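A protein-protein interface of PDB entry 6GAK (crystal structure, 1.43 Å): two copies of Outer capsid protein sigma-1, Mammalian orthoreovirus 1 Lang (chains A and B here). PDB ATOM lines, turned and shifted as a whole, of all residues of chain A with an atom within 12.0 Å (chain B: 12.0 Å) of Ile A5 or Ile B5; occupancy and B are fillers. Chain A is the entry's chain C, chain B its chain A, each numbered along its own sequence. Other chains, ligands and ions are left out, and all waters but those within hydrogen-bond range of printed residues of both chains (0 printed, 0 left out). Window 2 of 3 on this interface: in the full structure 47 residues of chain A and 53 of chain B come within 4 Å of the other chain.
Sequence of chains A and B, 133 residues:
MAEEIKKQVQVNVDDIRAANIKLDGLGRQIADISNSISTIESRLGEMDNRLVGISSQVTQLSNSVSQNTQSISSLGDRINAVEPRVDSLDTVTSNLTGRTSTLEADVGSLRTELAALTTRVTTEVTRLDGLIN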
ATOM      1  N   ALA A   2      24.630 -14.141  22.875  1.00  0.00           N
ATOM      2  CA  ALA A   2      25.597 -15.234  22.730  1.00  0.00           C
ATOM      3  C   ALA A   2      24.960 -16.440  22.049  1.00  0.00           C
ATOM      4  O   ALA A   2      25.549 -16.980  21.108  1.00  0.00           O
ATOM      5  CB  ALA A   2      26.176 -15.624  24.080  1.00  0.00           C
ATOM      6  N   GLU A   3      23.744 -16.850  22.499  1.00  0.00           N
ATOM      7  CA  GLU A   3      22.989 -17.943  21.892  1.00  0.00           C
ATOM      8  C   GLU A   3      22.599 -17.568  20.462  1.00  0.00           C
ATOM      9  O   GLU A   3      22.631 -18.399  19.544  1.00  0.00           O
ATOM     10  CB  GLU A   3      21.733 -18.252  22.748  1.00  0.00           C
ATOM     11  CG  GLU A   3      21.990 -19.325  23.792  1.00  0.00           C
ATOM     12  CD  GLU A   3      22.493 -20.651  23.245  1.00  0.00           C
ATOM     13  OE1 GLU A   3      21.895 -21.171  22.271  1.00  0.00           O
ATOM     14  OE2 GLU A   3      23.524 -21.139  23.765  1.00  0.00           O
ATOM     15  N   GLU A   4      22.290 -16.265  20.258  1.00  0.00           N
ATOM     16  CA  GLU A   4      21.951 -15.717  18.954  1.00  0.00           C
ATOM     17  C   GLU A   4      23.206 -15.832  18.065  1.00  0.00           C
ATOM     18  O   GLU A   4      23.088 -16.212  16.902  1.00  0.00           O
ATOM     19  CB  GLU A   4      21.589 -14.227  19.141  1.00  0.00           C
ATOM     20  CG  GLU A   4      20.921 -13.563  17.955  1.00  0.00           C
ATOM     21  N   ILE A   5      24.404 -15.512  18.645  1.00  0.00           N
ATOM     22  CA  ILE A   5      25.675 -15.532  17.915  1.00  0.00           C
ATOM     23  C   ILE A   5      25.975 -16.938  17.462  1.00  0.00           C
ATOM     24  O   ILE A   5      26.168 -17.158  16.278  1.00  0.00           O
ATOM     25  CB  ILE A   5      26.842 -14.899  18.745  1.00  0.00           C
ATOM     26  CG1 ILE A   5      26.584 -13.395  19.061  1.00  0.00           C
ATOM     27  CG2 ILE A   5      28.188 -15.068  18.078  1.00  0.00           C
ATOM     28  N   LYS A   6      25.970 -17.901  18.387  1.00  0.00           N
ATOM     29  CA  LYS A   6      26.275 -19.294  18.084  1.00  0.00           C
ATOM     30  C   LYS A   6      25.334 -19.842  16.973  1.00  0.00           C
ATOM     31  O   LYS A   6      25.785 -20.532  16.040  1.00  0.00           O
ATOM     32  CB  LYS A   6      26.122 -20.091  19.387  1.00  0.00           C
ATOM     33  CG  LYS A   6      26.345 -21.544  19.281  1.00  0.00           C
ATOM     34  CD  LYS A   6      26.166 -22.128  20.680  1.00  0.00           C
ATOM     35  CE  LYS A   6      26.174 -23.636  20.603  1.00  0.00           C
ATOM     36  NZ  LYS A   6      26.016 -24.259  21.941  1.00  0.00           N
ATOM     37  N   LYS A   7      24.054 -19.522  17.039  1.00  0.00           N
ATOM     38  CA  LYS A   7      23.096 -19.990  16.023  1.00  0.00           C
ATOM     39  C   LYS A   7      23.447 -19.421  14.625  1.00  0.00           C
ATOM     40  O   LYS A   7      23.425 -20.147  13.604  1.00  0.00           O
ATOM     41  CB  LYS A   7      21.652 -19.602  16.434  1.00  0.00           C
ATOM     42  CG  LYS A   7      21.113 -20.432  17.607  1.00  0.00           C
ATOM     43  CD  LYS A   7      19.760 -19.824  18.093  1.00  0.00           C
ATOM     44  CE  LYS A   7      19.281 -20.322  19.441  1.00  0.00           C
ATOM     45  NZ  LYS A   7      18.132 -19.506  19.992  1.00  0.00           N
ATOM     46  N   GLN A   8      23.767 -18.129  14.580  1.00  0.00           N
ATOM     47  CA  GLN A   8      24.081 -17.528  13.297  1.00  0.00           C
ATOM     48  C   GLN A   8      25.428 -18.065  12.727  1.00  0.00           C
ATOM     49  O   GLN A   8      25.612 -18.225  11.512  1.00  0.00           O
ATOM     50  CB  GLN A   8      24.185 -15.995  13.417  1.00  0.00           C
ATOM     51  CG  GLN A   8      24.340 -15.359  12.021  1.00  0.00           C
ATOM     52  CD  GLN A   8      23.178 -15.603  11.079  1.00  0.00           C
ATOM     53  OE1 GLN A   8      22.070 -15.131  11.338  1.00  0.00           O
ATOM     54  NE2 GLN A   8      23.412 -16.315   9.964  1.00  0.00           N
ATOM     55  N   VAL A   9      26.399 -18.315  13.595  1.00  0.00           N
ATOM     56  CA  VAL A   9      27.683 -18.844  13.133  1.00  0.00           C
ATOM     57  C   VAL A   9      27.435 -20.228  12.498  1.00  0.00           C
ATOM     58  O   VAL A   9      27.991 -20.507  11.414  1.00  0.00           O
ATOM     59  CB  VAL A   9      28.677 -18.925  14.322  1.00  0.00           C
ATOM     60  CG1 VAL A   9      29.929 -19.711  13.940  1.00  0.00           C
ATOM     61  CG2 VAL A   9      29.053 -17.520  14.878  1.00  0.00           C
ATOM     62  N   GLN A  10      26.544 -21.043  13.112  1.00  0.00           N
ATOM     63  CA  GLN A  10      26.239 -22.376  12.519  1.00  0.00           C
ATOM     64  C   GLN A  10      25.614 -22.218  11.155  1.00  0.00           C
ATOM     65  O   GLN A  10      26.022 -22.928  10.187  1.00  0.00           O
ATOM     66  CB  GLN A  10      25.316 -23.170  13.466  1.00  0.00           C
ATOM     67  CG  GLN A  10      24.881 -24.508  12.809  1.00  0.00           C
ATOM     68  CD  GLN A  10      26.035 -25.429  12.637  1.00  0.00           C
ATOM     69  OE1 GLN A  10      26.788 -25.668  13.598  1.00  0.00           O
ATOM     70  NE2 GLN A  10      25.974 -26.153  11.538  1.00  0.00           N
ATOM     71  N   VAL A  11      24.673 -21.282  11.029  1.00  0.00           N
ATOM     72  CA  VAL A  11      24.019 -21.010   9.737  1.00  0.00           C
ATOM     73  C   VAL A  11      25.094 -20.597   8.695  1.00  0.00           C
ATOM     74  O   VAL A  11      25.079 -21.101   7.556  1.00  0.00           O
ATOM     75  CB  VAL A  11      22.860 -19.998   9.848  1.00  0.00           C
ATOM     76  CG1 VAL A  11      22.469 -19.453   8.452  1.00  0.00           C
ATOM     77  CG2 VAL A  11      21.629 -20.658  10.537  1.00  0.00           C
ATOM     78  N   ASN A  12      26.063 -19.757   9.119  1.00  0.00           N
ATOM     79  CA  ASN A  12      27.148 -19.303   8.226  1.00  0.00           C
ATOM     80  C   ASN A  12      28.033 -20.445   7.791  1.00  0.00           C
ATOM     81  O   ASN A  12      28.345 -20.540   6.608  1.00  0.00           O
ATOM     82  CB  ASN A  12      27.933 -18.174   8.843  1.00  0.00           C
ATOM     83  CG  ASN A  12      27.133 -16.868   8.919  1.00  0.00           C
ATOM     84  OD1 ASN A  12      26.021 -16.732   8.392  1.00  0.00           O
ATOM     85  ND2 ASN A  12      27.728 -15.868   9.584  1.00  0.00           N
ATOM     86  N   VAL A  13      28.367 -21.390   8.714  1.00  0.00           N
ATOM     87  CA  VAL A  13      29.125 -22.597   8.322  1.00  0.00           C
ATOM     88  C   VAL A  13      28.402 -23.350   7.213  1.00  0.00           C
ATOM     89  O   VAL A  13      29.005 -23.721   6.190  1.00  0.00           O
ATOM     90  CB  VAL A  13      29.309 -23.512   9.580  1.00  0.00           C
ATOM     91  CG1 VAL A  13      29.912 -24.855   9.134  1.00  0.00           C
ATOM     92  CG2 VAL A  13      30.248 -22.834  10.570  1.00  0.00           C
ATOM     93  N   ASP A  14      27.095 -23.577   7.376  1.00  0.00           N
ATOM     94  CA  ASP A  14      26.332 -24.380   6.430  1.00  0.00           C
ATOM     95  C   ASP A  14      26.141 -23.634   5.116  1.00  0.00           C
ATOM     96  O   ASP A  14      26.214 -24.247   4.047  1.00  0.00           O
ATOM     97  CB  ASP A  14      25.018 -24.804   7.096  1.00  0.00           C
ATOM     98  CG  ASP A  14      25.266 -25.805   8.249  1.00  0.00           C
ATOM     99  OD1 ASP A  14      26.325 -26.475   8.246  1.00  0.00           O
ATOM    100  OD2 ASP A  14      24.559 -25.725   9.263  1.00  0.00           O
ATOM    101  N   ASP A  15      25.959 -22.324   5.180  1.00  0.00           N
ATOM    102  CA  ASP A  15      25.824 -21.529   3.950  1.00  0.00           C
ATOM    103  C   ASP A  15      27.122 -21.415   3.179  1.00  0.00           C
ATOM    104  O   ASP A  15      27.060 -21.439   1.933  1.00  0.00           O
ATOM    105  CB  ASP A  15      25.306 -20.133   4.295  1.00  0.00           C
ATOM    106  CG  ASP A  15      23.860 -20.072   4.735  1.00  0.00           C
ATOM    107  OD1 ASP A  15      23.134 -21.082   4.538  1.00  0.00           O
ATOM    108  OD2 ASP A  15      23.413 -18.988   5.120  1.00  0.00           O
ATOM    109  N   ILE A  16      28.280 -21.353   3.852  1.00  0.00           N
ATOM    110  CA  ILE A  16      29.568 -21.314   3.133  1.00  0.00           C
ATOM    111  C   ILE A  16      29.791 -22.665   2.426  1.00  0.00           C
ATOM    112  O   ILE A  16      30.195 -22.718   1.263  1.00  0.00           O
ATOM    113  CB  ILE A  16      30.698 -21.028   4.117  1.00  0.00           C
ATOM    114  CG1 ILE A  16      30.640 -19.552   4.605  1.00  0.00           C
ATOM    115  CG2 ILE A  16      32.075 -21.303   3.467  1.00  0.00           C
ATOM    116  CD1 ILE A  16      31.428 -19.286   5.852  1.00  0.00           C
ATOM    117  N   GLU B   3      29.806  -6.300  20.548  1.00  0.00           N
ATOM    118  CA  GLU B   3      31.115  -6.922  20.619  1.00  0.00           C
ATOM    119  C   GLU B   3      31.702  -7.028  19.193  1.00  0.00           C
ATOM    120  O   GLU B   3      30.960  -6.979  18.193  1.00  0.00           O
ATOM    121  CB  GLU B   3      31.042  -8.315  21.307  1.00  0.00           C
ATOM    122  CG  GLU B   3      30.593  -9.469  20.394  1.00  0.00           C
ATOM    123  N   GLU B   4      33.024  -7.226  19.115  1.00  0.00           N
ATOM    124  CA  GLU B   4      33.669  -7.387  17.818  1.00  0.00           C
ATOM    125  C   GLU B   4      33.200  -8.693  17.138  1.00  0.00           C
ATOM    126  O   GLU B   4      33.045  -8.713  15.927  1.00  0.00           O
ATOM    127  CB  GLU B   4      35.212  -7.325  17.896  1.00  0.00           C
ATOM    128  CG  GLU B   4      35.769  -5.910  17.811  1.00  0.00           C
ATOM    129  CD  GLU B   4      35.892  -5.269  16.430  1.00  0.00           C
ATOM    130  OE1 GLU B   4      37.018  -5.243  15.882  1.00  0.00           O
ATOM    131  OE2 GLU B   4      34.886  -4.710  15.939  1.00  0.00           O
ATOM    132  N   ILE B   5      32.923  -9.746  17.903  1.00  0.00           N
ATOM    133  CA  ILE B   5      32.419 -11.011  17.324  1.00  0.00           C
ATOM    134  C   ILE B   5      31.079 -10.802  16.626  1.00  0.00           C
ATOM    135  O   ILE B   5      30.924 -11.198  15.459  1.00  0.00           O
ATOM    136  CB  ILE B   5      32.333 -12.165  18.372  1.00  0.00           C
ATOM    137  CG1 ILE B   5      33.727 -12.421  19.032  1.00  0.00           C
ATOM    138  CG2 ILE B   5      31.763 -13.431  17.732  1.00  0.00           C
ATOM    139  CD1 ILE B   5      33.691 -13.271  20.318  1.00  0.00           C
ATOM    140  N   LYS B   6      30.115 -10.213  17.310  1.00  0.00           N
ATOM    141  CA  LYS B   6      28.784 -10.015  16.745  1.00  0.00           C
ATOM    142  C   LYS B   6      28.841  -9.205  15.407  1.00  0.00           C
ATOM    143  O   LYS B   6      28.175  -9.544  14.418  1.00  0.00           O
ATOM    144  CB  LYS B   6      27.919  -9.289  17.781  1.00  0.00           C
ATOM    145  CG  LYS B   6      26.493  -9.092  17.363  1.00  0.00           C
ATOM    146  CD  LYS B   6      25.744  -8.538  18.558  1.00  0.00           C
ATOM    147  CE  LYS B   6      24.325  -8.176  18.209  1.00  0.00           C
ATOM    148  NZ  LYS B   6      23.787  -7.135  19.137  1.00  0.00           N
ATOM    149  N   LYS B   7      29.692  -8.192  15.376  1.00  0.00           N
ATOM    150  CA  LYS B   7      29.878  -7.363  14.184  1.00  0.00           C
ATOM    151  C   LYS B   7      30.457  -8.176  13.027  1.00  0.00           C
ATOM    152  O   LYS B   7      29.980  -8.067  11.889  1.00  0.00           O
ATOM    153  CB  LYS B   7      30.824  -6.176  14.496  1.00  0.00           C
ATOM    154  CG  LYS B   7      30.181  -5.110  15.393  1.00  0.00           C
ATOM    155  CD  LYS B   7      31.245  -4.032  15.757  1.00  0.00           C
ATOM    156  CE  LYS B   7      30.689  -2.921  16.622  1.00  0.00           C
ATOM    157  NZ  LYS B   7      31.763  -1.936  17.054  1.00  0.00           N
ATOM    158  N   GLN B   8      31.468  -9.019  13.317  1.00  0.00           N
ATOM    159  CA  GLN B   8      32.072  -9.828  12.248  1.00  0.00           C
ATOM    160  C   GLN B   8      31.082 -10.882  11.747  1.00  0.00           C
ATOM    161  O   GLN B   8      31.095 -11.224  10.544  1.00  0.00           O
ATOM    162  CB  GLN B   8      33.355 -10.518  12.744  1.00  0.00           C
ATOM    163  CG  GLN B   8      34.103 -11.293  11.664  1.00  0.00           C
ATOM    164  CD  GLN B   8      34.582 -10.392  10.550  1.00  0.00           C
ATOM    165  OE1 GLN B   8      35.442  -9.529  10.760  1.00  0.00           O
ATOM    166  NE2 GLN B   8      34.047 -10.566   9.339  1.00  0.00           N
ATOM    167  N   VAL B   9      30.277 -11.465  12.665  1.00  0.00           N
ATOM    168  CA  VAL B   9      29.284 -12.469  12.215  1.00  0.00           C
ATOM    169  C   VAL B   9      28.295 -11.804  11.229  1.00  0.00           C
ATOM    170  O   VAL B   9      27.959 -12.398  10.187  1.00  0.00           O
ATOM    171  CB  VAL B   9      28.560 -13.066  13.444  1.00  0.00           C
ATOM    172  CG1 VAL B   9      27.398 -13.955  13.000  1.00  0.00           C
ATOM    173  CG2 VAL B   9      29.534 -13.857  14.286  1.00  0.00           C
ATOM    174  N   GLN B  10      27.894 -10.537  11.537  1.00  0.00           N
ATOM    175  CA  GLN B  10      26.976  -9.832  10.610  1.00  0.00           C
ATOM    176  C   GLN B  10      27.628  -9.507   9.277  1.00  0.00           C
ATOM    177  O   GLN B  10      27.035  -9.706   8.222  1.00  0.00           O
ATOM    178  CB  GLN B  10      26.414  -8.574  11.268  1.00  0.00           C
ATOM    179  CG  GLN B  10      25.365  -7.896  10.294  1.00  0.00           C
ATOM    180  CD  GLN B  10      24.179  -8.769   9.795  1.00  0.00           C
ATOM    181  OE1 GLN B  10      23.441  -9.387  10.585  1.00  0.00           O
ATOM    182  NE2 GLN B  10      23.828  -8.702   8.488  1.00  0.00           N
ATOM    183  N   VAL B  11      28.915  -9.092   9.302  1.00  0.00           N
ATOM    184  CA  VAL B  11      29.699  -8.867   8.071  1.00  0.00           C
ATOM    185  C   VAL B  11      29.750 -10.205   7.232  1.00  0.00           C
ATOM    186  O   VAL B  11      29.557 -10.167   6.028  1.00  0.00           O
ATOM    187  CB  VAL B  11      31.096  -8.333   8.422  1.00  0.00           C
ATOM    188  CG1 VAL B  11      32.037  -8.377   7.203  1.00  0.00           C
ATOM    189  CG2 VAL B  11      30.958  -6.875   8.889  1.00  0.00           C
ATOM    190  N   ASN B  12      29.952 -11.343   7.943  1.00  0.00           N
ATOM    191  CA  ASN B  12      29.955 -12.639   7.263  1.00  0.00           C
ATOM    192  C   ASN B  12      28.630 -12.967   6.640  1.00  0.00           C
ATOM    193  O   ASN B  12      28.627 -13.473   5.514  1.00  0.00           O
ATOM    194  CB  ASN B  12      30.455 -13.770   8.215  1.00  0.00           C
ATOM    195  CG  ASN B  12      31.938 -13.686   8.544  1.00  0.00           C
ATOM    196  OD1 ASN B  12      32.720 -12.863   7.961  1.00  0.00           O
ATOM    197  ND2 ASN B  12      32.356 -14.535   9.479  1.00  0.00           N
ATOM    198  N   VAL B  13      27.493 -12.671   7.341  1.00  0.00           N
ATOM    199  CA  VAL B  13      26.187 -12.878   6.727  1.00  0.00           C
ATOM    200  C   VAL B  13      26.132 -12.087   5.416  1.00  0.00           C
ATOM    201  O   VAL B  13      25.736 -12.586   4.371  1.00  0.00           O
ATOM    202  CB  VAL B  13      25.037 -12.423   7.699  1.00  0.00           C
ATOM    203  CG1 VAL B  13      23.696 -12.381   6.938  1.00  0.00           C
ATOM    204  CG2 VAL B  13      24.978 -13.369   8.906  1.00  0.00           C
ATOM    205  N   ASP B  14      26.513 -10.806   5.485  1.00  0.00           N
ATOM    206  CA  ASP B  14      26.388  -9.957   4.288  1.00  0.00           C
ATOM    207  C   ASP B  14      27.364 -10.430   3.170  1.00  0.00           C
ATOM    208  O   ASP B  14      26.973 -10.433   1.979  1.00  0.00           O
ATOM    209  CB  ASP B  14      26.611  -8.471   4.610  1.00  0.00           C
ATOM    210  CG  ASP B  14      25.544  -7.896   5.552  1.00  0.00           C
ATOM    211  OD1 ASP B  14      24.377  -8.392   5.533  1.00  0.00           O
ATOM    212  OD2 ASP B  14      25.879  -7.008   6.349  1.00  0.00           O
ATOM    213  N   ASP B  15      28.599 -10.876   3.571  1.00  0.00           N
ATOM    214  CA  ASP B  15      29.535 -11.328   2.546  1.00  0.00           C
ATOM    215  C   ASP B  15      29.098 -12.642   1.893  1.00  0.00           C
ATOM    216  O   ASP B  15      29.321 -12.824   0.691  1.00  0.00           O
ATOM    217  CB  ASP B  15      30.940 -11.436   3.096  1.00  0.00           C
ATOM    218  CG  ASP B  15      31.541 -10.115   3.460  1.00  0.00           C
ATOM    219  OD1 ASP B  15      30.983  -9.043   3.019  1.00  0.00           O
ATOM    220  OD2 ASP B  15      32.617 -10.117   4.084  1.00  0.00           O
ATOM    221  N   ILE B  16      28.424 -13.528   2.667  1.00  0.00           N
ATOM    222  CA  ILE B  16      27.946 -14.784   2.087  1.00  0.00           C
ATOM    223  C   ILE B  16      26.794 -14.480   1.104  1.00  0.00           C
ATOM    224  O   ILE B  16      26.726 -15.055   0.021  1.00  0.00           O
ATOM    225  CB  ILE B  16      27.499 -15.732   3.209  1.00  0.00           C
ATOM    226  CG1 ILE B  16      28.715 -16.273   4.013  1.00  0.00           C
ATOM    227  CG2 ILE B  16      26.669 -16.902   2.624  1.00  0.00           C
ATOM    228  CD1 ILE B  16      28.214 -16.825   5.418  1.00  0.00           C
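CG2 of Ile B5 touches CG2 of Ile A5, at 3.9 Å. Gln A8 touches Val B9. Gln A8 touches Val B13. Val A9 touches Val B9 (CG2 to CG2, 3.7 Å). Asn A12 touches Val B9 (ND2 to O, 3.5 Å). CB of Asn B12 touches ND2 of Asn A12 (3.7 Å). Val B13 touches Asn A12. CD1 of Ile B16 touches CG of Asn A12 (3.7 Å). CB of Asp A15 touches CG2 of Ile B16, at 3.9 Å. Ile A16 touches Ile B16.
Hydrophobic or aromatic side chains of chain B that line the printed part of chain A: Ile B5, Val B9, Val B13 and Ile B16. Of the 15 printed residues of chain A, 6 touch a printed residue of chain B. Hydrophobic or aromatic side chains of chain A that line the printed part of chain B: Ile A5, Val A9 and Ile A16. Among the printed residues, 10 pairs touch across the chains.
Ile A5 touches its own counterpart, Ile B5. Gln A8 touches Val B9, but with the chains exchanged Val A9 does not touch Gln B8 (7.6 Å). Val B9 touches its own counterpart, Val A9. Asn A12 touches its own counterpart, Asn B12. Of the 10 pairs that touch across the chains among the printed residues, 4 have their exchanged pair printed and touching as well.
Ala A2 touches none of the printed residues of chain B. No residue of chain B comes within 4 Å of Glu A4. Of chain B, only Ile B5 comes within 4 Å of Ile A5. Gln A8 touches just these residues of chain B: Val B9 (3.5 Å) and Val B13 (3.5 Å). Of chain B, only Val B9 comes within 4 Å of Val A9. Of the printed residues of chain B, Asp A15 touches Ile B16 (3.9 Å). Glu B3 touches none of the printed residues of chain A. No residue of chain A comes within 4 Å of Glu B4. Of the printed residues of chain A, Ile B5 touches Ile A5. No residue of chain A comes within 4 Å of Lys B6. Lys B7 touches none of the printed residues of chain A. No residue of chain A comes within 4 Å of Gln B8. Val B9 touches three residues of chain A. Val B11 touches none of the printed residues of chain A. Of the printed residues of chain A, Asn B12 touches Asn A12. Asp B14 touches none of the printed residues of chain A. Of the printed residues of chain A, Ile B16 touches Asn A12 (3.7 Å), Asp A15 (3.9 Å) and Ile A16 (3.7 Å). The nearest printed residue of chain A that does not touch Asn B12 is Ile A16 (6.0 Å).
The side-chain amide nitrogen (NE2) of Gln A8 lies within hydrogen-bond range of the side-chain amide oxygen (OD1) of Asn A12, at 3.1 Å. NE2 of Gln B8 is in hydrogen-bond range of OD1 of Asn B12 (3.0 Å).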
